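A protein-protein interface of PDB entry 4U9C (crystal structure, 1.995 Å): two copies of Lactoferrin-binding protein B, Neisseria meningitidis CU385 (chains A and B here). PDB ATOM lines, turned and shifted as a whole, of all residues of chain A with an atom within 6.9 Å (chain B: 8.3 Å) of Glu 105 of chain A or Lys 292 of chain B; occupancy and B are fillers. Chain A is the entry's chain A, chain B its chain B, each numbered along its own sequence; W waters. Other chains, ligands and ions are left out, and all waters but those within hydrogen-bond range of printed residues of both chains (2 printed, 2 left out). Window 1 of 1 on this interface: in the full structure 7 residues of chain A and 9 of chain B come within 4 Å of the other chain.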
ATOM      1  N   ARG A  52      21.477  29.998  -4.630  1.00  0.00           N
ATOM      2  CA  ARG A  52      20.271  29.205  -4.838  1.00  0.00           C
ATOM      3  C   ARG A  52      19.988  28.329  -3.606  1.00  0.00           C
ATOM      4  O   ARG A  52      20.893  27.887  -2.910  1.00  0.00           O
ATOM      5  CB  ARG A  52      20.406  28.326  -6.085  1.00  0.00           C
ATOM      6  CG  ARG A  52      19.052  27.852  -6.641  1.00  0.00           C
ATOM      7  CD  ARG A  52      19.191  27.203  -8.027  1.00  0.00           C
ATOM      8  NE  ARG A  52      17.897  26.919  -8.660  1.00  0.00           N
ATOM      9  CZ  ARG A  52      17.737  26.710  -9.958  1.00  0.00           C
ATOM     10  NH1 ARG A  52      18.784  26.773 -10.785  1.00  0.00           N
ATOM     11  NH2 ARG A  52      16.535  26.441 -10.433  1.00  0.00           N
ATOM     12  N   LYS A  98      16.962  37.405 -14.531  1.00  0.00           N
ATOM     13  CA  LYS A  98      17.798  36.232 -14.730  1.00  0.00           C
ATOM     14  C   LYS A  98      17.470  35.167 -13.691  1.00  0.00           C
ATOM     15  O   LYS A  98      17.430  33.975 -13.992  1.00  0.00           O
ATOM     16  CB  LYS A  98      19.273  36.629 -14.645  1.00  0.00           C
ATOM     17  CG  LYS A  98      19.726  37.461 -15.843  1.00  0.00           C
ATOM     18  CD  LYS A  98      21.140  37.999 -15.699  1.00  0.00           C
ATOM     19  CE  LYS A  98      21.532  38.853 -16.903  1.00  0.00           C
ATOM     20  NZ  LYS A  98      22.947  39.313 -16.851  1.00  0.00           N
ATOM     21  N   LYS A 100      14.580  34.910 -11.977  1.00  0.00           N
ATOM     22  CA  LYS A 100      13.242  34.418 -12.252  1.00  0.00           C
ATOM     23  C   LYS A 100      13.271  33.437 -13.422  1.00  0.00           C
ATOM     24  O   LYS A 100      12.578  32.413 -13.399  1.00  0.00           O
ATOM     25  CB  LYS A 100      12.296  35.568 -12.540  1.00  0.00           C
ATOM     26  CG  LYS A 100      10.928  35.088 -12.957  1.00  0.00           C
ATOM     27  CD  LYS A 100       9.912  36.208 -13.009  1.00  0.00           C
ATOM     28  CE  LYS A 100       8.529  35.652 -13.301  1.00  0.00           C
ATOM     29  NZ  LYS A 100       8.518  34.878 -14.578  1.00  0.00           N
ATOM     30  N   LYS A 101      14.080  33.748 -14.433  1.00  0.00           N
ATOM     31  CA  LYS A 101      14.256  32.860 -15.581  1.00  0.00           C
ATOM     32  C   LYS A 101      14.728  31.462 -15.162  1.00  0.00           C
ATOM     33  O   LYS A 101      14.204  30.459 -15.640  1.00  0.00           O
ATOM     34  CB  LYS A 101      15.268  33.443 -16.569  1.00  0.00           C
ATOM     35  CG  LYS A 101      15.524  32.533 -17.781  1.00  0.00           C
ATOM     36  CD  LYS A 101      16.840  32.836 -18.483  1.00  0.00           C
ATOM     37  CE  LYS A 101      18.023  32.510 -17.550  1.00  0.00           C
ATOM     38  NZ  LYS A 101      19.315  32.300 -18.249  1.00  0.00           N
ATOM     39  N   LYS A 102      15.737  31.392 -14.294  1.00  0.00           N
ATOM     40  CA  LYS A 102      16.258  30.105 -13.857  1.00  0.00           C
ATOM     41  C   LYS A 102      15.184  29.294 -13.145  1.00  0.00           C
ATOM     42  O   LYS A 102      15.103  28.067 -13.297  1.00  0.00           O
ATOM     43  CB  LYS A 102      17.474  30.282 -12.949  1.00  0.00           C
ATOM     44  CG  LYS A 102      18.699  30.784 -13.686  1.00  0.00           C
ATOM     45  CD  LYS A 102      19.914  30.818 -12.793  1.00  0.00           C
ATOM     46  CE  LYS A 102      21.177  30.858 -13.621  1.00  0.00           C
ATOM     47  NZ  LYS A 102      21.434  29.558 -14.308  1.00  0.00           N
ATOM     48  N   ILE A 103      14.363  29.964 -12.352  1.00  0.00           N
ATOM     49  CA  ILE A 103      13.256  29.253 -11.732  1.00  0.00           C
ATOM     50  C   ILE A 103      12.331  28.708 -12.816  1.00  0.00           C
ATOM     51  O   ILE A 103      11.961  27.534 -12.776  1.00  0.00           O
ATOM     52  CB  ILE A 103      12.459  30.141 -10.765  1.00  0.00           C
ATOM     53  CG1 ILE A 103      13.394  30.584  -9.620  1.00  0.00           C
ATOM     54  CG2 ILE A 103      11.199  29.392 -10.271  1.00  0.00           C
ATOM     55  CD1 ILE A 103      12.714  30.954  -8.335  1.00  0.00           C
ATOM     56  N   ASN A 104      12.005  29.542 -13.803  1.00  0.00           N
ATOM     57  CA  ASN A 104      11.049  29.151 -14.833  1.00  0.00           C
ATOM     58  C   ASN A 104      11.623  28.078 -15.744  1.00  0.00           C
ATOM     59  O   ASN A 104      10.884  27.323 -16.360  1.00  0.00           O
ATOM     60  CB  ASN A 104      10.607  30.352 -15.681  1.00  0.00           C
ATOM     61  CG  ASN A 104       9.576  31.228 -14.978  1.00  0.00           C
ATOM     62  OD1 ASN A 104       9.687  32.453 -14.987  1.00  0.00           O
ATOM     63  ND2 ASN A 104       8.569  30.604 -14.371  1.00  0.00           N
ATOM     64  N   GLU A 105      12.943  28.027 -15.835  1.00  0.00           N
ATOM     65  CA  GLU A 105      13.611  26.970 -16.585  1.00  0.00           C
ATOM     66  C   GLU A 105      13.385  25.603 -15.930  1.00  0.00           C
ATOM     67  O   GLU A 105      13.422  24.570 -16.601  1.00  0.00           O
ATOM     68  CB  GLU A 105      15.097  27.289 -16.712  1.00  0.00           C
ATOM     69  CG  GLU A 105      15.359  28.273 -17.853  1.00  0.00           C
ATOM     70  CD  GLU A 105      16.736  28.882 -17.832  1.00  0.00           C
ATOM     71  OE1 GLU A 105      17.562  28.512 -16.965  1.00  0.00           O
ATOM     72  OE2 GLU A 105      17.005  29.711 -18.724  1.00  0.00           O
ATOM     73  N   ARG A 106      13.165  25.597 -14.618  1.00  0.00           N
ATOM     74  CA  ARG A 106      12.888  24.354 -13.896  1.00  0.00           C
ATOM     75  C   ARG A 106      11.407  24.043 -13.943  1.00  0.00           C
ATOM     76  O   ARG A 106      11.028  22.900 -14.152  1.00  0.00           O
ATOM     77  CB  ARG A 106      13.361  24.431 -12.442  1.00  0.00           C
ATOM     78  CG  ARG A 106      13.080  23.163 -11.650  1.00  0.00           C
ATOM     79  CD  ARG A 106      13.759  23.169 -10.283  1.00  0.00           C
ATOM     80  NE  ARG A 106      13.433  21.948  -9.561  1.00  0.00           N
ATOM     81  CZ  ARG A 106      13.506  21.807  -8.245  1.00  0.00           C
ATOM     82  NH1 ARG A 106      13.887  22.825  -7.478  1.00  0.00           N
ATOM     83  NH2 ARG A 106      13.179  20.643  -7.696  1.00  0.00           N
ATOM     84  N   TYR A 107      10.584  25.079 -13.788  1.00  0.00           N
ATOM     85  CA  TYR A 107       9.129  24.951 -13.821  1.00  0.00           C
ATOM     86  C   TYR A 107       8.516  26.097 -14.603  1.00  0.00           C
ATOM     87  O   TYR A 107       8.524  27.231 -14.131  1.00  0.00           O
ATOM     88  CB  TYR A 107       8.531  25.020 -12.420  1.00  0.00           C
ATOM     89  CG  TYR A 107       9.044  24.051 -11.399  1.00  0.00           C
ATOM     90  CD1 TYR A 107       8.711  22.715 -11.456  1.00  0.00           C
ATOM     91  CD2 TYR A 107       9.825  24.496 -10.338  1.00  0.00           C
ATOM     92  CE1 TYR A 107       9.157  21.842 -10.512  1.00  0.00           C
ATOM     93  CE2 TYR A 107      10.279  23.636  -9.386  1.00  0.00           C
ATOM     94  CZ  TYR A 107       9.941  22.301  -9.472  1.00  0.00           C
ATOM     95  OH  TYR A 107      10.389  21.402  -8.522  1.00  0.00           O
ATOM     96  N   SER A 108       7.948  25.827 -15.768  1.00  0.00           N
ATOM     97  CA  SER A 108       7.406  26.907 -16.586  1.00  0.00           C
ATOM     98  C   SER A 108       6.148  27.558 -15.969  1.00  0.00           C
ATOM     99  O   SER A 108       5.856  28.732 -16.231  1.00  0.00           O
ATOM    100  CB  SER A 108       7.095  26.372 -17.994  1.00  0.00           C
ATOM    101  OG  SER A 108       6.184  25.282 -17.952  1.00  0.00           O
ATOM    102  N   LEU B 267      27.016  11.605 -15.708  1.00  0.00           N
ATOM    103  CA  LEU B 267      26.025  12.658 -15.557  1.00  0.00           C
ATOM    104  C   LEU B 267      24.816  12.315 -16.409  1.00  0.00           C
ATOM    105  O   LEU B 267      24.934  12.157 -17.616  1.00  0.00           O
ATOM    106  CB  LEU B 267      26.584  14.015 -15.999  1.00  0.00           C
ATOM    107  CG  LEU B 267      25.591  15.186 -16.024  1.00  0.00           C
ATOM    108  CD1 LEU B 267      25.101  15.470 -14.602  1.00  0.00           C
ATOM    109  CD2 LEU B 267      26.162  16.454 -16.637  1.00  0.00           C
ATOM    110  N   THR B 268      23.661  12.163 -15.783  1.00  0.00           N
ATOM    111  CA  THR B 268      22.446  11.918 -16.533  1.00  0.00           C
ATOM    112  C   THR B 268      22.029  13.178 -17.281  1.00  0.00           C
ATOM    113  O   THR B 268      21.813  14.245 -16.676  1.00  0.00           O
ATOM    114  CB  THR B 268      21.312  11.445 -15.610  1.00  0.00           C
ATOM    115  OG1 THR B 268      21.683  10.198 -15.008  1.00  0.00           O
ATOM    116  CG2 THR B 268      20.007  11.272 -16.384  1.00  0.00           C
ATOM    117  N   ILE B 269      21.901  13.054 -18.598  1.00  0.00           N
ATOM    118  CA  ILE B 269      21.431  14.157 -19.426  1.00  0.00           C
ATOM    119  C   ILE B 269      19.902  14.096 -19.610  1.00  0.00           C
ATOM    120  O   ILE B 269      19.218  15.074 -19.320  1.00  0.00           O
ATOM    121  CB  ILE B 269      22.116  14.143 -20.805  1.00  0.00           C
ATOM    122  CG1 ILE B 269      23.639  14.246 -20.666  1.00  0.00           C
ATOM    123  CG2 ILE B 269      21.626  15.301 -21.658  1.00  0.00           C
ATOM    124  CD1 ILE B 269      24.142  15.487 -19.950  1.00  0.00           C
ATOM    125  N   LYS B 286      13.342  13.678 -20.927  1.00  0.00           N
ATOM    126  CA  LYS B 286      13.312  14.909 -20.139  1.00  0.00           C
ATOM    127  C   LYS B 286      14.683  15.238 -19.598  1.00  0.00           C
ATOM    128  O   LYS B 286      15.373  14.378 -19.046  1.00  0.00           O
ATOM    129  CB  LYS B 286      12.302  14.802 -19.003  1.00  0.00           C
ATOM    130  CG  LYS B 286      10.869  14.798 -19.525  1.00  0.00           C
ATOM    131  CD  LYS B 286       9.856  14.813 -18.405  1.00  0.00           C
ATOM    132  CE  LYS B 286       8.456  15.101 -18.927  1.00  0.00           C
ATOM    133  NZ  LYS B 286       7.415  14.468 -18.069  1.00  0.00           N
ATOM    134  N   VAL B 287      15.077  16.491 -19.780  1.00  0.00           N
ATOM    135  CA  VAL B 287      16.338  16.957 -19.255  1.00  0.00           C
ATOM    136  C   VAL B 287      16.325  16.821 -17.751  1.00  0.00           C
ATOM    137  O   VAL B 287      15.377  17.239 -17.079  1.00  0.00           O
ATOM    138  CB  VAL B 287      16.609  18.412 -19.631  1.00  0.00           C
ATOM    139  CG1 VAL B 287      17.945  18.859 -19.030  1.00  0.00           C
ATOM    140  CG2 VAL B 287      16.598  18.557 -21.145  1.00  0.00           C
ATOM    141  N   SER B 288      17.372  16.216 -17.227  1.00  0.00           N
ATOM    142  CA  SER B 288      17.505  16.059 -15.799  1.00  0.00           C
ATOM    143  C   SER B 288      17.646  17.408 -15.121  1.00  0.00           C
ATOM    144  O   SER B 288      18.315  18.317 -15.614  1.00  0.00           O
ATOM    145  CB  SER B 288      18.714  15.192 -15.470  1.00  0.00           C
ATOM    146  OG  SER B 288      19.876  15.926 -15.762  1.00  0.00           O
ATOM    147  N   THR B 289      17.042  17.493 -13.956  1.00  0.00           N
ATOM    148  CA  THR B 289      17.106  18.670 -13.113  1.00  0.00           C
ATOM    149  C   THR B 289      18.552  19.007 -12.802  1.00  0.00           C
ATOM    150  O   THR B 289      18.940  20.179 -12.762  1.00  0.00           O
ATOM    151  CB  THR B 289      16.324  18.436 -11.803  1.00  0.00           C
ATOM    152  OG1 THR B 289      14.924  18.269 -12.104  1.00  0.00           O
ATOM    153  CG2 THR B 289      16.512  19.597 -10.819  1.00  0.00           C
ATOM    154  N   GLU B 290      19.349  17.970 -12.582  1.00  0.00           N
ATOM    155  CA  GLU B 290      20.767  18.153 -12.263  1.00  0.00           C
ATOM    156  C   GLU B 290      21.496  18.952 -13.360  1.00  0.00           C
ATOM    157  O   GLU B 290      22.298  19.832 -13.058  1.00  0.00           O
ATOM    158  CB  GLU B 290      21.441  16.806 -12.050  1.00  0.00           C
ATOM    159  CG  GLU B 290      22.912  16.952 -11.707  1.00  0.00           C
ATOM    160  CD  GLU B 290      23.535  15.662 -11.228  1.00  0.00           C
ATOM    161  OE1 GLU B 290      23.052  14.574 -11.628  1.00  0.00           O
ATOM    162  OE2 GLU B 290      24.509  15.743 -10.450  1.00  0.00           O
ATOM    163  N   VAL B 291      21.213  18.651 -14.623  1.00  0.00           N
ATOM    164  CA  VAL B 291      21.792  19.402 -15.728  1.00  0.00           C
ATOM    165  C   VAL B 291      21.403  20.886 -15.604  1.00  0.00           C
ATOM    166  O   VAL B 291      22.242  21.768 -15.777  1.00  0.00           O
ATOM    167  CB  VAL B 291      21.325  18.851 -17.091  1.00  0.00           C
ATOM    168  CG1 VAL B 291      21.574  19.854 -18.210  1.00  0.00           C
ATOM    169  CG2 VAL B 291      22.013  17.536 -17.383  1.00  0.00           C
ATOM    170  N   LYS B 292      20.134  21.153 -15.294  1.00  0.00           N
ATOM    171  CA  LYS B 292      19.624  22.526 -15.231  1.00  0.00           C
ATOM    172  C   LYS B 292      20.281  23.342 -14.118  1.00  0.00           C
ATOM    173  O   LYS B 292      20.617  24.507 -14.305  1.00  0.00           O
ATOM    174  CB  LYS B 292      18.114  22.517 -15.017  1.00  0.00           C
ATOM    175  CG  LYS B 292      17.328  21.769 -16.091  1.00  0.00           C
ATOM    176  CD  LYS B 292      15.846  22.047 -15.986  1.00  0.00           C
ATOM    177  CE  LYS B 292      15.019  21.226 -16.980  1.00  0.00           C
ATOM    178  NZ  LYS B 292      13.590  21.655 -16.973  1.00  0.00           N
ATOM    179  N   THR B 293      20.490  22.719 -12.966  1.00  0.00           N
ATOM    180  CA  THR B 293      20.887  23.447 -11.775  1.00  0.00           C
ATOM    181  C   THR B 293      22.396  23.445 -11.555  1.00  0.00           C
ATOM    182  O   THR B 293      22.938  24.396 -10.997  1.00  0.00           O
ATOM    183  CB  THR B 293      20.191  22.861 -10.533  1.00  0.00           C
ATOM    184  OG1 THR B 293      20.554  21.483 -10.372  1.00  0.00           O
ATOM    185  CG2 THR B 293      18.682  22.972 -10.696  1.00  0.00           C
ATOM    186  N   GLN B 294      23.070  22.394 -12.001  1.00  0.00           N
ATOM    187  CA  GLN B 294      24.500  22.240 -11.725  1.00  0.00           C
ATOM    188  C   GLN B 294      25.350  22.391 -12.980  1.00  0.00           C
ATOM    189  O   GLN B 294      26.567  22.412 -12.882  1.00  0.00           O
ATOM    190  CB  GLN B 294      24.780  20.870 -11.095  1.00  0.00           C
ATOM    191  CG  GLN B 294      23.995  20.593  -9.821  1.00  0.00           C
ATOM    192  CD  GLN B 294      24.376  21.502  -8.680  1.00  0.00           C
ATOM    193  OE1 GLN B 294      25.548  21.616  -8.325  1.00  0.00           O
ATOM    194  NE2 GLN B 294      23.380  22.167  -8.101  1.00  0.00           N
ATOM    195  N   HIS B 295      24.720  22.482 -14.151  1.00  0.00           N
ATOM    196  CA  HIS B 295      25.467  22.577 -15.415  1.00  0.00           C
ATOM    197  C   HIS B 295      24.848  23.595 -16.369  1.00  0.00           C
ATOM    198  O   HIS B 295      24.867  23.416 -17.591  1.00  0.00           O
ATOM    199  CB  HIS B 295      25.537  21.191 -16.068  1.00  0.00           C
ATOM    200  CG  HIS B 295      26.114  20.152 -15.160  1.00  0.00           C
ATOM    201  ND1 HIS B 295      27.462  19.874 -15.107  1.00  0.00           N
ATOM    202  CD2 HIS B 295      25.531  19.369 -14.222  1.00  0.00           C
ATOM    203  CE1 HIS B 295      27.681  18.947 -14.191  1.00  0.00           C
ATOM    204  NE2 HIS B 295      26.526  18.629 -13.635  1.00  0.00           N
ATOM    205  N   ALA B 296      24.347  24.686 -15.788  1.00  0.00           N
ATOM    206  CA  ALA B 296      23.646  25.735 -16.524  1.00  0.00           C
ATOM    207  C   ALA B 296      24.514  26.428 -17.577  1.00  0.00           C
ATOM    208  O   ALA B 296      23.991  26.921 -18.575  1.00  0.00           O
ATOM    209  CB  ALA B 296      23.102  26.766 -15.549  1.00  0.00           C
ATOM    210  N   ASP B 297      25.822  26.480 -17.332  1.00  0.00           N
ATOM    211  CA  ASP B 297      26.761  27.208 -18.190  1.00  0.00           C
ATOM    212  C   ASP B 297      27.475  26.321 -19.185  1.00  0.00           C
ATOM    213  O   ASP B 297      28.339  26.792 -19.920  1.00  0.00           O
ATOM    214  CB  ASP B 297      27.801  27.952 -17.361  1.00  0.00           C
ATOM    215  CG  ASP B 297      27.175  28.872 -16.344  1.00  0.00           C
ATOM    216  OD1 ASP B 297      26.083  29.399 -16.644  1.00  0.00           O
ATOM    217  OD2 ASP B 297      27.768  29.068 -15.257  1.00  0.00           O
ATOM    218  N   LYS B 298      27.136  25.035 -19.198  1.00  0.00           N
ATOM    219  CA  LYS B 298      27.729  24.115 -20.157  1.00  0.00           C
ATOM    220  C   LYS B 298      26.677  23.192 -20.788  1.00  0.00           C
ATOM    221  O   LYS B 298      26.058  23.553 -21.791  1.00  0.00           O
ATOM    222  CB  LYS B 298      28.815  23.271 -19.475  1.00  0.00           C
ATOM    223  CG  LYS B 298      29.573  22.342 -20.430  1.00  0.00           C
ATOM    224  CD  LYS B 298      30.629  21.525 -19.682  1.00  0.00           C
ATOM    225  CE  LYS B 298      32.024  22.010 -19.933  1.00  0.00           C
ATOM    226  NZ  LYS B 298      33.010  21.009 -19.433  1.00  0.00           N
ATOM    227  N   GLU B 299      26.460  22.021 -20.192  1.00  0.00           N
ATOM    228  CA  GLU B 299      25.573  21.017 -20.783  1.00  0.00           C
ATOM    229  C   GLU B 299      24.156  21.550 -21.031  1.00  0.00           C
ATOM    230  O   GLU B 299      23.504  21.150 -21.984  1.00  0.00           O
ATOM    231  CB  GLU B 299      25.503  19.764 -19.908  1.00  0.00           C
ATOM    232  CG  GLU B 299      26.692  18.809 -20.026  1.00  0.00           C
ATOM    233  CD  GLU B 299      27.882  19.225 -19.189  1.00  0.00           C
ATOM    234  OE1 GLU B 299      27.857  20.340 -18.619  1.00  0.00           O
ATOM    235  OE2 GLU B 299      28.829  18.414 -19.073  1.00  0.00           O
ATOM    236  N   TYR B 300      23.680  22.418 -20.148  1.00  0.00           N
ATOM    237  CA  TYR B 300      22.326  22.956 -20.253  1.00  0.00           C
ATOM    238  C   TYR B 300      22.162  23.839 -21.499  1.00  0.00           C
ATOM    239  O   TYR B 300      21.065  23.948 -22.071  1.00  0.00           O
ATOM    240  CB  TYR B 300      21.971  23.746 -18.982  1.00  0.00           C
ATOM    241  CG  TYR B 300      20.567  24.318 -19.031  1.00  0.00           C
ATOM    242  CD1 TYR B 300      19.448  23.487 -19.026  1.00  0.00           C
ATOM    243  CD2 TYR B 300      20.371  25.685 -19.142  1.00  0.00           C
ATOM    244  CE1 TYR B 300      18.151  24.023 -19.100  1.00  0.00           C
ATOM    245  CE2 TYR B 300      19.110  26.219 -19.225  1.00  0.00           C
ATOM    246  CZ  TYR B 300      18.001  25.394 -19.206  1.00  0.00           C
ATOM    247  OH  TYR B 300      16.756  25.963 -19.292  1.00  0.00           O
ATOM    248  N   LEU B 301      23.254  24.448 -21.947  1.00  0.00           N
ATOM    249  CA  LEU B 301      23.204  25.312 -23.129  1.00  0.00           C
ATOM    250  C   LEU B 301      22.865  24.517 -24.398  1.00  0.00           C
ATOM    251  O   LEU B 301      22.480  25.102 -25.412  1.00  0.00           O
ATOM    252  CB  LEU B 301      24.534  26.043 -23.299  1.00  0.00           C
ATOM    253  CG  LEU B 301      24.941  26.964 -22.143  1.00  0.00           C
ATOM    254  CD1 LEU B 301      26.196  27.730 -22.511  1.00  0.00           C
ATOM    255  CD2 LEU B 301      23.806  27.939 -21.735  1.00  0.00           C
ATOM    256  N   PHE B 303      21.381  20.958 -23.893  1.00  0.00           N
ATOM    257  CA  PHE B 303      20.268  20.125 -23.472  1.00  0.00           C
ATOM    258  C   PHE B 303      19.380  20.890 -22.488  1.00  0.00           C
ATOM    259  O   PHE B 303      19.608  20.867 -21.280  1.00  0.00           O
ATOM    260  CB  PHE B 303      20.795  18.827 -22.850  1.00  0.00           C
ATOM    261  CG  PHE B 303      21.846  18.134 -23.694  1.00  0.00           C
ATOM    262  CD1 PHE B 303      21.495  17.461 -24.854  1.00  0.00           C
ATOM    263  CD2 PHE B 303      23.174  18.149 -23.314  1.00  0.00           C
ATOM    264  CE1 PHE B 303      22.450  16.831 -25.624  1.00  0.00           C
ATOM    265  CE2 PHE B 303      24.138  17.519 -24.079  1.00  0.00           C
ATOM    266  CZ  PHE B 303      23.776  16.856 -25.235  1.00  0.00           C
ATOM    267  N   HIS B 304      18.364  21.565 -23.016  1.00  0.00           N
ATOM    268  CA  HIS B 304      17.556  22.478 -22.215  1.00  0.00           C
ATOM    269  C   HIS B 304      16.056  22.285 -22.368  1.00  0.00           C
ATOM    270  O   HIS B 304      15.308  22.816 -21.568  1.00  0.00           O
ATOM    271  CB  HIS B 304      17.884  23.939 -22.560  1.00  0.00           C
ATOM    272  CG  HIS B 304      17.886  24.231 -24.026  1.00  0.00           C
ATOM    273  ND1 HIS B 304      16.728  24.370 -24.773  1.00  0.00           N
ATOM    274  CD2 HIS B 304      18.912  24.400 -24.892  1.00  0.00           C
ATOM    275  CE1 HIS B 304      17.047  24.620 -26.027  1.00  0.00           C
ATOM    276  NE2 HIS B 304      18.367  24.641 -26.129  1.00  0.00           N
ATOM    277  N   THR B 305      15.620  21.538 -23.377  1.00  0.00           N
ATOM    278  CA  THR B 305      14.189  21.356 -23.632  1.00  0.00           C
ATOM    279  C   THR B 305      13.835  19.867 -23.713  1.00  0.00           C
ATOM    280  O   THR B 305      14.568  19.080 -24.302  1.00  0.00           O
ATOM    281  CB  THR B 305      13.778  22.072 -24.930  1.00  0.00           C
ATOM    282  OG1 THR B 305      14.124  23.459 -24.826  1.00  0.00           O
ATOM    283  CG2 THR B 305      12.283  21.966 -25.179  1.00  0.00           C
ATOM    284  N   ASP B 306      12.697  19.491 -23.138  1.00  0.00           N
ATOM    285  CA  ASP B 306      12.261  18.088 -23.132  1.00  0.00           C
ATOM    286  C   ASP B 306      11.800  17.661 -24.524  1.00  0.00           C
ATOM    287  O   ASP B 306      11.583  18.500 -25.396  1.00  0.00           O
ATOM    288  CB  ASP B 306      11.112  17.875 -22.140  1.00  0.00           C
ATOM    289  CG  ASP B 306      11.476  18.259 -20.712  1.00  0.00           C
ATOM    290  OD1 ASP B 306      12.670  18.216 -20.364  1.00  0.00           O
ATOM    291  OD2 ASP B 306      10.548  18.582 -19.927  1.00  0.00           O
HETATM  292  O   HOH W   1      21.593  26.851 -10.238  1.00  0.00           O
HETATM  293  O   HOH W   2      14.982  24.125 -19.160  1.00  0.00           O
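Water W2 lies within hydrogen-bond range of OH of Tyr 300 of chain B (2.6 Å), O of His 304 of chain B (2.8 Å) and O of Glu 105 of chain A (3.0 Å). Water W1 lies within hydrogen-bond range of NH1 of Arg 52 of chain A and O of Thr 293 of chain B.
The side-chain amino group of Lys 101 of chain A is in salt-bridge range of the side-chain carboxylate of Glu 105 of chain A (3.5 Å). O of Thr 289 of chain B is in hydrogen-bond range of OG1 of Thr 293 of chain B. The backbone NH (N) of Tyr 300 of chain B is in hydrogen-bond range of the backbone carbonyl oxygen (O) of His 295 of chain B (3.0 Å).
No position is printed for both chains.
Of chain B, only Lys 292 (2.9 Å) and Tyr 300 (3.1 Å) come within 4 Å of Glu 105 of chain A. Printed residues of chain A within 4 Å of Lys 292 of chain B: Glu 105 (2.9 Å). Of the printed residues of chain B, Arg 52 of chain A touches Thr 293 (3.8 Å). Of the printed residues of chain A, Thr 293 of chain B touches Arg 52. Of the printed residues of chain B, Lys 102 of chain A touches Ala 296. Of the printed residues of chain A, Tyr 300 of chain B touches Glu 105 (3.1 Å). Printed residues of chain A within 4 Å of Ala 296 of chain B: Lys 102.
Arg 52 of chain A touches Thr 293 of chain B (NH1 to CG2, 3.8 Å). NZ of Lys 102 of chain A touches CB of Ala 296 of chain B (3.5 Å). Glu 105 of chain A touches Tyr 300 of chain B.
Of the 11 printed residues of chain A, 3 touch a printed residue of chain B. Hydrophobic or aromatic side chains of chain B within 4 Å of the printed part of chain A: Ala 296 and Tyr 300. Among the printed residues, 4 pairs touch across the chains. Among the printed residues, no Asp or Glu carboxylate lies within 4 Å of a Lys or Arg side-chain nitrogen of the other chain.
The backbone carbonyl oxygen of Glu 105 of chain A sits at hydrogen-bond distance from the side-chain amino group of Lys 292 of chain B, 2.9 Å away.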
